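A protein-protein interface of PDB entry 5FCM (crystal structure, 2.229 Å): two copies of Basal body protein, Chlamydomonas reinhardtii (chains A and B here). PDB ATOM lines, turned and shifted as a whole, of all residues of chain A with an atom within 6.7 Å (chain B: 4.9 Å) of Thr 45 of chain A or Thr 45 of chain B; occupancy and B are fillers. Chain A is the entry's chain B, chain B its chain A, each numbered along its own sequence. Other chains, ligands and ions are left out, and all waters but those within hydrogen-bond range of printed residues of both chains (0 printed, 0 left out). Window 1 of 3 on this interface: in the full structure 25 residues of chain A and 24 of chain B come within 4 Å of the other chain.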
ATOM      1  N   GLU A  40     -11.386   3.134 -34.848  1.00  0.00           N
ATOM      2  CA  GLU A  40     -10.152   2.866 -34.127  1.00  0.00           C
ATOM      3  C   GLU A  40     -10.438   2.353 -32.719  1.00  0.00           C
ATOM      4  O   GLU A  40      -9.871   1.350 -32.292  1.00  0.00           O
ATOM      5  CB  GLU A  40      -9.292   4.125 -34.069  1.00  0.00           C
ATOM      6  CG  GLU A  40      -8.759   4.554 -35.423  1.00  0.00           C
ATOM      7  CD  GLU A  40      -8.230   5.971 -35.417  1.00  0.00           C
ATOM      8  OE1 GLU A  40      -8.255   6.609 -34.343  1.00  0.00           O
ATOM      9  OE2 GLU A  40      -7.793   6.448 -36.485  1.00  0.00           O
ATOM     10  N   ASP A  41     -11.319   3.041 -32.002  1.00  0.00           N
ATOM     11  CA  ASP A  41     -11.667   2.645 -30.642  1.00  0.00           C
ATOM     12  C   ASP A  41     -12.334   1.279 -30.625  1.00  0.00           C
ATOM     13  O   ASP A  41     -12.046   0.450 -29.765  1.00  0.00           O
ATOM     14  CB  ASP A  41     -12.586   3.683 -30.002  1.00  0.00           C
ATOM     15  CG  ASP A  41     -11.854   4.954 -29.632  1.00  0.00           C
ATOM     16  OD1 ASP A  41     -10.683   5.104 -30.042  1.00  0.00           O
ATOM     17  OD2 ASP A  41     -12.449   5.805 -28.937  1.00  0.00           O
ATOM     18  N   LEU A  42     -13.227   1.050 -31.580  1.00  0.00           N
ATOM     19  CA  LEU A  42     -13.947  -0.212 -31.663  1.00  0.00           C
ATOM     20  C   LEU A  42     -12.978  -1.372 -31.857  1.00  0.00           C
ATOM     21  O   LEU A  42     -13.126  -2.425 -31.236  1.00  0.00           O
ATOM     22  CB  LEU A  42     -14.962  -0.175 -32.806  1.00  0.00           C
ATOM     23  CG  LEU A  42     -15.757  -1.462 -33.047  1.00  0.00           C
ATOM     24  CD1 LEU A  42     -16.627  -1.804 -31.842  1.00  0.00           C
ATOM     25  CD2 LEU A  42     -16.603  -1.338 -34.304  1.00  0.00           C
ATOM     26  N   VAL A  43     -11.989  -1.176 -32.721  1.00  0.00           N
ATOM     27  CA  VAL A  43     -11.023  -2.225 -33.019  1.00  0.00           C
ATOM     28  C   VAL A  43     -10.066  -2.397 -31.844  1.00  0.00           C
ATOM     29  O   VAL A  43      -9.762  -3.519 -31.447  1.00  0.00           O
ATOM     30  CB  VAL A  43     -10.258  -1.919 -34.323  1.00  0.00           C
ATOM     31  CG1 VAL A  43      -9.115  -2.909 -34.537  1.00  0.00           C
ATOM     32  CG2 VAL A  43     -11.211  -1.955 -35.504  1.00  0.00           C
ATOM     33  N   HIS A  44      -9.597  -1.285 -31.287  1.00  0.00           N
ATOM     34  CA  HIS A  44      -8.662  -1.341 -30.171  1.00  0.00           C
ATOM     35  C   HIS A  44      -9.291  -2.046 -28.973  1.00  0.00           C
ATOM     36  O   HIS A  44      -8.661  -2.894 -28.342  1.00  0.00           O
ATOM     37  CB  HIS A  44      -8.208   0.062 -29.773  1.00  0.00           C
ATOM     38  CG  HIS A  44      -7.258   0.079 -28.617  1.00  0.00           C
ATOM     39  ND1 HIS A  44      -6.012  -0.507 -28.667  1.00  0.00           N
ATOM     40  CD2 HIS A  44      -7.376   0.606 -27.374  1.00  0.00           C
ATOM     41  CE1 HIS A  44      -5.401  -0.338 -27.509  1.00  0.00           C
ATOM     42  NE2 HIS A  44      -6.206   0.334 -26.707  1.00  0.00           N
ATOM     43  N   THR A  45     -10.534  -1.696 -28.663  1.00  0.00           N
ATOM     44  CA  THR A  45     -11.229  -2.297 -27.532  1.00  0.00           C
ATOM     45  C   THR A  45     -11.506  -3.777 -27.792  1.00  0.00           C
ATOM     46  O   THR A  45     -11.485  -4.588 -26.867  1.00  0.00           O
ATOM     47  CB  THR A  45     -12.556  -1.574 -27.234  1.00  0.00           C
ATOM     48  OG1 THR A  45     -12.316  -0.171 -27.075  1.00  0.00           O
ATOM     49  CG2 THR A  45     -13.185  -2.114 -25.957  1.00  0.00           C
ATOM     50  N   THR A  46     -11.763  -4.127 -29.050  1.00  0.00           N
ATOM     51  CA  THR A  46     -12.033  -5.515 -29.409  1.00  0.00           C
ATOM     52  C   THR A  46     -10.762  -6.349 -29.274  1.00  0.00           C
ATOM     53  O   THR A  46     -10.812  -7.500 -28.843  1.00  0.00           O
ATOM     54  CB  THR A  46     -12.587  -5.638 -30.845  1.00  0.00           C
ATOM     55  OG1 THR A  46     -13.820  -4.916 -30.948  1.00  0.00           O
ATOM     56  CG2 THR A  46     -12.841  -7.100 -31.214  1.00  0.00           C
ATOM     57  N   ASP A  47      -9.626  -5.767 -29.647  1.00  0.00           N
ATOM     58  CA  ASP A  47      -8.342  -6.442 -29.508  1.00  0.00           C
ATOM     59  C   ASP A  47      -8.055  -6.727 -28.042  1.00  0.00           C
ATOM     60  O   ASP A  47      -7.680  -7.841 -27.677  1.00  0.00           O
ATOM     61  CB  ASP A  47      -7.211  -5.600 -30.103  1.00  0.00           C
ATOM     62  CG  ASP A  47      -7.183  -5.644 -31.617  1.00  0.00           C
ATOM     63  OD1 ASP A  47      -7.641  -6.652 -32.194  1.00  0.00           O
ATOM     64  OD2 ASP A  47      -6.693  -4.669 -32.229  1.00  0.00           O
ATOM     65  N   SER A  48      -8.230  -5.710 -27.205  1.00  0.00           N
ATOM     66  CA  SER A  48      -7.987  -5.846 -25.775  1.00  0.00           C
ATOM     67  C   SER A  48      -8.915  -6.898 -25.177  1.00  0.00           C
ATOM     68  O   SER A  48      -8.486  -7.739 -24.389  1.00  0.00           O
ATOM     69  CB  SER A  48      -8.176  -4.503 -25.066  1.00  0.00           C
ATOM     70  OG  SER A  48      -7.300  -3.521 -25.596  1.00  0.00           O
ATOM     71  N   TYR A  49     -10.187  -6.844 -25.559  1.00  0.00           N
ATOM     72  CA  TYR A  49     -11.161  -7.837 -25.124  1.00  0.00           C
ATOM     73  C   TYR A  49     -10.660  -9.243 -25.432  1.00  0.00           C
ATOM     74  O   TYR A  49     -10.587 -10.097 -24.548  1.00  0.00           O
ATOM     75  CB  TYR A  49     -12.511  -7.594 -25.804  1.00  0.00           C
ATOM     76  CG  TYR A  49     -13.496  -8.732 -25.647  1.00  0.00           C
ATOM     77  CD1 TYR A  49     -14.323  -8.813 -24.536  1.00  0.00           C
ATOM     78  CD2 TYR A  49     -13.605  -9.720 -26.615  1.00  0.00           C
ATOM     79  CE1 TYR A  49     -15.227  -9.851 -24.391  1.00  0.00           C
ATOM     80  CE2 TYR A  49     -14.505 -10.760 -26.480  1.00  0.00           C
ATOM     81  CZ  TYR A  49     -15.313 -10.820 -25.367  1.00  0.00           C
ATOM     82  OH  TYR A  49     -16.210 -11.855 -25.230  1.00  0.00           O
ATOM     83  N   THR A  50     -10.313  -9.472 -26.693  1.00  0.00           N
ATOM     84  CA  THR A  50      -9.837 -10.776 -27.134  1.00  0.00           C
ATOM     85  C   THR A  50      -8.600 -11.195 -26.345  1.00  0.00           C
ATOM     86  O   THR A  50      -8.465 -12.354 -25.958  1.00  0.00           O
ATOM     87  CB  THR A  50      -9.510 -10.768 -28.641  1.00  0.00           C
ATOM     88  OG1 THR A  50     -10.673 -10.375 -29.380  1.00  0.00           O
ATOM     89  CG2 THR A  50      -9.064 -12.146 -29.109  1.00  0.00           C
ATOM     90  N   MET B   3     -17.006 -12.565 -32.453  1.00  0.00           N
ATOM     91  CA  MET B   3     -16.988 -11.239 -31.847  1.00  0.00           C
ATOM     92  C   MET B   3     -16.141 -10.296 -32.698  1.00  0.00           C
ATOM     93  O   MET B   3     -16.613  -9.245 -33.138  1.00  0.00           O
ATOM     94  CB  MET B   3     -16.448 -11.312 -30.419  1.00  0.00           C
ATOM     95  CG  MET B   3     -16.944 -10.203 -29.501  1.00  0.00           C
ATOM     96  SD  MET B   3     -16.044  -8.649 -29.670  1.00  0.00           S
ATOM     97  CE  MET B   3     -16.547  -7.813 -28.168  1.00  0.00           C
ATOM     98  N   VAL B   7     -17.295  -7.429 -35.631  1.00  0.00           N
ATOM     99  CA  VAL B   7     -16.639  -6.162 -35.918  1.00  0.00           C
ATOM    100  C   VAL B   7     -16.182  -6.159 -37.369  1.00  0.00           C
ATOM    101  O   VAL B   7     -16.367  -5.176 -38.089  1.00  0.00           O
ATOM    102  CB  VAL B   7     -15.452  -5.917 -34.965  1.00  0.00           C
ATOM    103  CG1 VAL B   7     -14.716  -4.628 -35.329  1.00  0.00           C
ATOM    104  CG2 VAL B   7     -15.932  -5.869 -33.524  1.00  0.00           C
ATOM    105  N   ASP B  41     -22.159  -0.167 -30.945  1.00  0.00           N
ATOM    106  CA  ASP B  41     -21.232  -1.290 -31.041  1.00  0.00           C
ATOM    107  C   ASP B  41     -20.069  -1.095 -30.070  1.00  0.00           C
ATOM    108  O   ASP B  41     -19.675  -2.022 -29.359  1.00  0.00           O
ATOM    109  CB  ASP B  41     -20.703  -1.440 -32.470  1.00  0.00           C
ATOM    110  CG  ASP B  41     -21.764  -1.927 -33.442  1.00  0.00           C
ATOM    111  OD1 ASP B  41     -22.762  -2.525 -32.990  1.00  0.00           O
ATOM    112  OD2 ASP B  41     -21.594  -1.718 -34.662  1.00  0.00           O
ATOM    113  N   LEU B  42     -19.532   0.120 -30.046  1.00  0.00           N
ATOM    114  CA  LEU B  42     -18.411   0.455 -29.176  1.00  0.00           C
ATOM    115  C   LEU B  42     -18.809   0.354 -27.704  1.00  0.00           C
ATOM    116  O   LEU B  42     -18.014  -0.077 -26.868  1.00  0.00           O
ATOM    117  CB  LEU B  42     -17.899   1.862 -29.495  1.00  0.00           C
ATOM    118  CG  LEU B  42     -16.766   2.417 -28.628  1.00  0.00           C
ATOM    119  CD1 LEU B  42     -15.541   1.514 -28.666  1.00  0.00           C
ATOM    120  CD2 LEU B  42     -16.408   3.823 -29.081  1.00  0.00           C
ATOM    121  N   VAL B  43     -20.041   0.748 -27.394  1.00  0.00           N
ATOM    122  CA  VAL B  43     -20.545   0.677 -26.025  1.00  0.00           C
ATOM    123  C   VAL B  43     -20.607  -0.780 -25.573  1.00  0.00           C
ATOM    124  O   VAL B  43     -20.087  -1.133 -24.514  1.00  0.00           O
ATOM    125  CB  VAL B  43     -21.928   1.356 -25.900  1.00  0.00           C
ATOM    126  CG1 VAL B  43     -22.564   1.070 -24.536  1.00  0.00           C
ATOM    127  CG2 VAL B  43     -21.805   2.856 -26.117  1.00  0.00           C
ATOM    128  N   HIS B  44     -21.247  -1.620 -26.380  1.00  0.00           N
ATOM    129  CA  HIS B  44     -21.410  -3.030 -26.049  1.00  0.00           C
ATOM    130  C   HIS B  44     -20.055  -3.714 -25.901  1.00  0.00           C
ATOM    131  O   HIS B  44     -19.836  -4.481 -24.963  1.00  0.00           O
ATOM    132  CB  HIS B  44     -22.245  -3.735 -27.119  1.00  0.00           C
ATOM    133  CG  HIS B  44     -23.652  -3.232 -27.214  1.00  0.00           C
ATOM    134  ND1 HIS B  44     -24.181  -2.329 -26.318  1.00  0.00           N
ATOM    135  CD2 HIS B  44     -24.640  -3.507 -28.099  1.00  0.00           C
ATOM    136  CE1 HIS B  44     -25.435  -2.069 -26.646  1.00  0.00           C
ATOM    137  NE2 HIS B  44     -25.737  -2.770 -27.723  1.00  0.00           N
ATOM    138  N   THR B  45     -19.149  -3.430 -26.830  1.00  0.00           N
ATOM    139  CA  THR B  45     -17.811  -4.009 -26.802  1.00  0.00           C
ATOM    140  C   THR B  45     -17.059  -3.541 -25.562  1.00  0.00           C
ATOM    141  O   THR B  45     -16.307  -4.302 -24.956  1.00  0.00           O
ATOM    142  CB  THR B  45     -17.016  -3.639 -28.075  1.00  0.00           C
ATOM    143  OG1 THR B  45     -17.567  -4.333 -29.200  1.00  0.00           O
ATOM    144  CG2 THR B  45     -15.545  -4.013 -27.942  1.00  0.00           C
ATOM    145  N   THR B  46     -17.268  -2.285 -25.190  1.00  0.00           N
ATOM    146  CA  THR B  46     -16.620  -1.723 -24.013  1.00  0.00           C
ATOM    147  C   THR B  46     -17.195  -2.350 -22.743  1.00  0.00           C
ATOM    148  O   THR B  46     -16.487  -2.517 -21.751  1.00  0.00           O
ATOM    149  CB  THR B  46     -16.783  -0.196 -23.964  1.00  0.00           C
ATOM    150  OG1 THR B  46     -16.239   0.378 -25.157  1.00  0.00           O
ATOM    151  CG2 THR B  46     -16.065   0.389 -22.758  1.00  0.00           C
ATOM    152  N   ASP B  47     -18.479  -2.693 -22.782  1.00  0.00           N
ATOM    153  CA  ASP B  47     -19.124  -3.372 -21.663  1.00  0.00           C
ATOM    154  C   ASP B  47     -18.538  -4.768 -21.492  1.00  0.00           C
ATOM    155  O   ASP B  47     -18.182  -5.173 -20.387  1.00  0.00           O
ATOM    156  CB  ASP B  47     -20.639  -3.469 -21.877  1.00  0.00           C
ATOM    157  CG  ASP B  47     -21.328  -2.117 -21.836  1.00  0.00           C
ATOM    158  OD1 ASP B  47     -20.715  -1.142 -21.352  1.00  0.00           O
ATOM    159  OD2 ASP B  47     -22.492  -2.036 -22.280  1.00  0.00           O
ATOM    160  N   SER B  48     -18.452  -5.500 -22.598  1.00  0.00           N
ATOM    161  CA  SER B  48     -17.911  -6.853 -22.588  1.00  0.00           C
ATOM    162  C   SER B  48     -16.475  -6.865 -22.082  1.00  0.00           C
ATOM    163  O   SER B  48     -16.094  -7.716 -21.280  1.00  0.00           O
ATOM    164  CB  SER B  48     -17.977  -7.462 -23.989  1.00  0.00           C
ATOM    165  OG  SER B  48     -19.316  -7.550 -24.439  1.00  0.00           O
ATOM    166  N   TYR B  49     -15.683  -5.914 -22.559  1.00  0.00           N
ATOM    167  CA  TYR B  49     -14.295  -5.786 -22.142  1.00  0.00           C
ATOM    168  C   TYR B  49     -14.208  -5.568 -20.634  1.00  0.00           C
ATOM    169  O   TYR B  49     -13.341  -6.131 -19.965  1.00  0.00           O
ATOM    170  CB  TYR B  49     -13.630  -4.634 -22.896  1.00  0.00           C
ATOM    171  CG  TYR B  49     -12.182  -4.397 -22.537  1.00  0.00           C
ATOM    172  CD1 TYR B  49     -11.291  -5.455 -22.412  1.00  0.00           C
ATOM    173  CD2 TYR B  49     -11.699  -3.108 -22.350  1.00  0.00           C
ATOM    174  CE1 TYR B  49      -9.965  -5.237 -22.092  1.00  0.00           C
ATOM    175  CE2 TYR B  49     -10.375  -2.881 -22.033  1.00  0.00           C
ATOM    176  CZ  TYR B  49      -9.512  -3.948 -21.904  1.00  0.00           C
ATOM    177  OH  TYR B  49      -8.192  -3.727 -21.587  1.00  0.00           O
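O of Asp 41 of chain B lies within hydrogen-bond range of OG1 of Thr 45 of chain B (3.1 Å).
O of Leu 42 of chain B sits at hydrogen-bond distance from OG1 of Thr 46 of chain B (2.5 Å).
The side-chain hydroxyl (OG) of Ser 48 of chain B lies within hydrogen-bond range of the backbone carbonyl oxygen (O) of His 44 of chain B, at 3.2 Å.
OG1 of Thr 45 of chain A is in hydrogen-bond range of O of Asp 41 of chain A (2.8 Å).
The backbone carbonyl oxygen (O) of Leu 42 of chain A sits at hydrogen-bond distance from the side-chain hydroxyl (OG1) of Thr 46 of chain A, 2.6 Å away.
OG1 of Thr 50 of chain A lies within hydrogen-bond range of O of Thr 46 of chain A (2.9 Å).
Among the printed residues, pairs that only touch across the chains: Asp 41 of chain A with Leu 42 of chain B (3.8 Å), Leu 42 of chain A with Val 7 of chain B (3.9 Å), Leu 42 of chain A with Asp 41 of chain B (3.9 Å), Leu 42 of chain A with Leu 42 of chain B (3.7 Å), Leu 42 of chain A with Thr 45 of chain B (3.8 Å), Thr 45 of chain A with Leu 42 of chain B (3.97 Å), Thr 45 of chain A with Thr 45 of chain B (3.6 Å), Thr 45 of chain A with Thr 46 of chain B (3.97 Å), Thr 45 of chain A with Tyr 49 of chain B (3.99 Å), Thr 46 of chain A with Met 3 of chain B (3.9 Å), Thr 46 of chain A with Val 7 of chain B (3.5 Å), Thr 46 of chain A with Thr 45 of chain B (3.6 Å), Ser 48 of chain A with Tyr 49 of chain B (3.5 Å), Tyr 49 of chain A with Met 3 of chain B (3.8 Å), Tyr 49 of chain A with Ser 48 of chain B (3.7 Å) and Tyr 49 of chain A with Tyr 49 of chain B (3.6 Å).
Glu 40 of chain A touches none of the printed residues of chain B.
Of the printed residues of chain B, Asp 41 of chain A touches Leu 42.
Of the printed residues of chain B, Thr 45 of chain A touches Leu 42 (3.97 Å), Thr 45 (3.6 Å), Thr 46 (3.97 Å) and Tyr 49 (3.99 Å).
Printed residues of chain B within 4 Å of Ser 48 of chain A: Tyr 49.
Of the printed residues of chain B, Tyr 49 of chain A touches Met 3, Ser 48 and Tyr 49.
Thr 45 of chain B touches three residues of chain A.
Of the printed residues of chain A, Thr 46 of chain B touches Thr 45 (3.97 Å).
Printed residues of chain A within 4 Å of Tyr 49 of chain B: Thr 45 (3.99 Å), Ser 48 (3.5 Å) and Tyr 49 (3.6 Å).
The nearest residue of chain A that does not touch Thr 45 of chain B is Tyr 49 of chain A (4.9 Å).
Of the 11 printed residues of chain A, 6 touch a printed residue of chain B.
Hydrophobic or aromatic side chains of chain A that line the printed part of chain B: Leu 42 and Tyr 49.
Along chain A the printed residues that touch a printed residue of chain B span positions 41 to 49.
Among the printed residues, 16 pairs touch across the chains.
Asp 41 of chain A touches Leu 42 of chain B, and with the chains exchanged Leu 42 of chain A touches Asp 41 of chain B.
Leu 42 of chain B touches its own counterpart, Leu 42 of chain A.
Ser 48 of chain A touches Tyr 49 of chain B, and with the chains exchanged Tyr 49 of chain A touches Ser 48 of chain B.
Tyr 49 of chain A touches its own counterpart, Tyr 49 of chain B.
Of the 16 pairs that touch across the chains among the printed residues, 11 have their exchanged pair printed and touching as well.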
